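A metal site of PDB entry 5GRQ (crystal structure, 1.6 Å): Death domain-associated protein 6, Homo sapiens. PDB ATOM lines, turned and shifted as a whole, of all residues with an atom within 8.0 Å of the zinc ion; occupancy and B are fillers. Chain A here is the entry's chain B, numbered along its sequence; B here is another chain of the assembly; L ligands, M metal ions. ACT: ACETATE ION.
The nearest printed residue that does not touch the zinc ion is Phe 45 (4.5 Å).
A ring nitrogen (ND1) of His 83 sits at hydrogen-bond distance from the backbone carbonyl oxygen (O) of Val 79 (2.8 Å).
The backbone NH (N) of Glu 50 sits close to the side-chain hydroxyl (OG) of Ser 48 (3.5 Å).
The zinc ion is bound by N of Gly 1 of chain B (2.0 Å), NE2 of His 83 (2.0 Å), OXT of the ligand (2.0 Å) and OE2 of Glu 50 (2.1 Å).
The zinc ion has four donor atoms within binding distance.
Slightly farther from the zinc ion lies the side-chain carboxylate (OE1) of Glu 50 (2.8 Å).
Slightly farther from the zinc ion lies O of the ligand (2.8 Å).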
ATOM      1  N   PHE A  45       1.110 -17.119 -18.778  1.00  0.00           N
ATOM      2  CA  PHE A  45       1.679 -16.007 -19.541  1.00  0.00           C
ATOM      3  C   PHE A  45       2.483 -15.070 -18.640  1.00  0.00           C
ATOM      4  O   PHE A  45       3.587 -14.658 -18.986  1.00  0.00           O
ATOM      5  CB  PHE A  45       0.571 -15.220 -20.245  1.00  0.00           C
ATOM      6  CG  PHE A  45       1.088 -14.028 -21.012  1.00  0.00           C
ATOM      7  CD1 PHE A  45       1.706 -14.208 -22.232  1.00  0.00           C
ATOM      8  CD2 PHE A  45       0.953 -12.738 -20.500  1.00  0.00           C
ATOM      9  CE1 PHE A  45       2.173 -13.108 -22.951  1.00  0.00           C
ATOM     10  CE2 PHE A  45       1.420 -11.638 -21.218  1.00  0.00           C
ATOM     11  CZ  PHE A  45       2.034 -11.824 -22.446  1.00  0.00           C
ATOM     12  N   SER A  48       6.036 -16.331 -18.055  1.00  0.00           N
ATOM     13  CA  SER A  48       6.618 -16.933 -19.255  1.00  0.00           C
ATOM     14  C   SER A  48       7.807 -16.148 -19.796  1.00  0.00           C
ATOM     15  O   SER A  48       7.934 -14.947 -19.587  1.00  0.00           O
ATOM     16  CB  SER A  48       5.563 -17.050 -20.347  1.00  0.00           C
ATOM     17  OG  SER A  48       5.175 -15.774 -20.835  1.00  0.00           O
ATOM     18  N   GLU A  50       7.965 -15.798 -22.940  1.00  0.00           N
ATOM     19  CA  GLU A  50       7.259 -14.993 -23.936  1.00  0.00           C
ATOM     20  C   GLU A  50       6.982 -13.586 -23.430  1.00  0.00           C
ATOM     21  O   GLU A  50       7.292 -12.597 -24.105  1.00  0.00           O
ATOM     22  CB  GLU A  50       5.960 -15.702 -24.314  1.00  0.00           C
ATOM     23  CG  GLU A  50       5.079 -14.896 -25.274  1.00  0.00           C
ATOM     24  CD  GLU A  50       3.686 -15.453 -25.432  1.00  0.00           C
ATOM     25  OE1 GLU A  50       3.216 -16.226 -24.562  1.00  0.00           O
ATOM     26  OE2 GLU A  50       3.035 -15.083 -26.426  1.00  0.00           O
ATOM     27  N   PHE A  51       6.423 -13.479 -22.216  1.00  0.00           N
ATOM     28  CA  PHE A  51       6.131 -12.155 -21.662  1.00  0.00           C
ATOM     29  C   PHE A  51       7.410 -11.393 -21.328  1.00  0.00           C
ATOM     30  O   PHE A  51       7.476 -10.175 -21.524  1.00  0.00           O
ATOM     31  CB  PHE A  51       5.234 -12.314 -20.438  1.00  0.00           C
ATOM     32  CG  PHE A  51       4.606 -11.024 -19.949  1.00  0.00           C
ATOM     33  CD1 PHE A  51       4.340  -9.977 -20.827  1.00  0.00           C
ATOM     34  CD2 PHE A  51       4.265 -10.880 -18.614  1.00  0.00           C
ATOM     35  CE1 PHE A  51       3.746  -8.804 -20.364  1.00  0.00           C
ATOM     36  CE2 PHE A  51       3.674  -9.701 -18.144  1.00  0.00           C
ATOM     37  CZ  PHE A  51       3.417  -8.677 -19.024  1.00  0.00           C
ATOM     38  N   ILE A  54       8.645  -9.899 -24.521  1.00  0.00           N
ATOM     39  CA  ILE A  54       7.745  -8.806 -24.874  1.00  0.00           C
ATOM     40  C   ILE A  54       8.086  -7.546 -24.075  1.00  0.00           C
ATOM     41  O   ILE A  54       8.166  -6.441 -24.644  1.00  0.00           O
ATOM     42  CB  ILE A  54       6.283  -9.238 -24.676  1.00  0.00           C
ATOM     43  CG1 ILE A  54       5.860 -10.128 -25.850  1.00  0.00           C
ATOM     44  CG2 ILE A  54       5.343  -8.035 -24.536  1.00  0.00           C
ATOM     45  CD1 ILE A  54       4.602 -10.945 -25.597  1.00  0.00           C
ATOM     46  N   VAL A  79      -1.809  -7.316 -26.466  1.00  0.00           N
ATOM     47  CA  VAL A  79      -1.175  -8.586 -26.091  1.00  0.00           C
ATOM     48  C   VAL A  79      -1.730  -9.080 -24.752  1.00  0.00           C
ATOM     49  O   VAL A  79      -2.071 -10.258 -24.605  1.00  0.00           O
ATOM     50  CB  VAL A  79       0.352  -8.418 -26.045  1.00  0.00           C
ATOM     51  CG1 VAL A  79       0.987  -9.615 -25.345  1.00  0.00           C
ATOM     52  CG2 VAL A  79       0.916  -8.206 -27.448  1.00  0.00           C
ATOM     53  N   ALA A  82      -5.185 -10.434 -25.145  1.00  0.00           N
ATOM     54  CA  ALA A  82      -5.196 -11.722 -25.839  1.00  0.00           C
ATOM     55  C   ALA A  82      -4.845 -12.874 -24.915  1.00  0.00           C
ATOM     56  O   ALA A  82      -5.198 -14.022 -25.211  1.00  0.00           O
ATOM     57  CB  ALA A  82      -4.214 -11.690 -27.014  1.00  0.00           C
ATOM     58  N   HIS A  83      -4.128 -12.612 -23.816  1.00  0.00           N
ATOM     59  CA  HIS A  83      -3.764 -13.634 -22.847  1.00  0.00           C
ATOM     60  C   HIS A  83      -4.612 -13.519 -21.575  1.00  0.00           C
ATOM     61  O   HIS A  83      -4.195 -13.992 -20.511  1.00  0.00           O
ATOM     62  CB  HIS A  83      -2.275 -13.543 -22.544  1.00  0.00           C
ATOM     63  CG  HIS A  83      -1.392 -13.834 -23.725  1.00  0.00           C
ATOM     64  ND1 HIS A  83      -1.055 -12.882 -24.657  1.00  0.00           N
ATOM     65  CD2 HIS A  83      -0.791 -14.974 -24.119  1.00  0.00           C
ATOM     66  CE1 HIS A  83      -0.269 -13.422 -25.578  1.00  0.00           C
ATOM     67  NE2 HIS A  83      -0.082 -14.694 -25.268  1.00  0.00           N
ATOM     68  N   GLY B   1       0.542 -17.709 -25.805  1.00  0.00           N
ATOM     69  CA  GLY B   1       1.576 -18.715 -25.847  1.00  0.00           C
ATOM     70  C   GLY B   1       0.989 -20.071 -25.517  1.00  0.00           C
ATOM     71  O   GLY B   1      -0.101 -20.408 -25.969  1.00  0.00           O
ATOM     72  N   LYS B   2       1.693 -20.844 -24.717  1.00  0.00           N
ATOM     73  CA  LYS B   2       1.184 -22.159 -24.355  1.00  0.00           C
ATOM     74  C   LYS B   2      -0.075 -22.043 -23.499  1.00  0.00           C
ATOM     75  O   LYS B   2      -0.360 -21.009 -22.888  1.00  0.00           O
ATOM     76  CB  LYS B   2       2.270 -22.963 -23.667  1.00  0.00           C
ATOM     77  CG  LYS B   2       3.325 -23.415 -24.696  1.00  0.00           C
ATOM     78  CD  LYS B   2       4.547 -24.082 -24.116  1.00  0.00           C
ATOM     79  CE  LYS B   2       5.485 -24.482 -25.243  1.00  0.00           C
ATOM     80  NZ  LYS B   2       6.844 -24.864 -24.749  1.00  0.00           N
HETATM   81  C   ACT L   1       1.128 -16.239 -29.032  1.00  0.00           C
HETATM   82  O   ACT L   1       2.017 -17.082 -28.761  1.00  0.00           O
HETATM   83  OXT ACT L   1       0.503 -15.488 -28.267  1.00  0.00           O
HETATM   84  CH3 ACT L   1       0.764 -16.114 -30.548  1.00  0.00           C
HETATM   85 ZN    ZN M   1       1.147 -15.886 -26.364  1.00  0.00          ZN
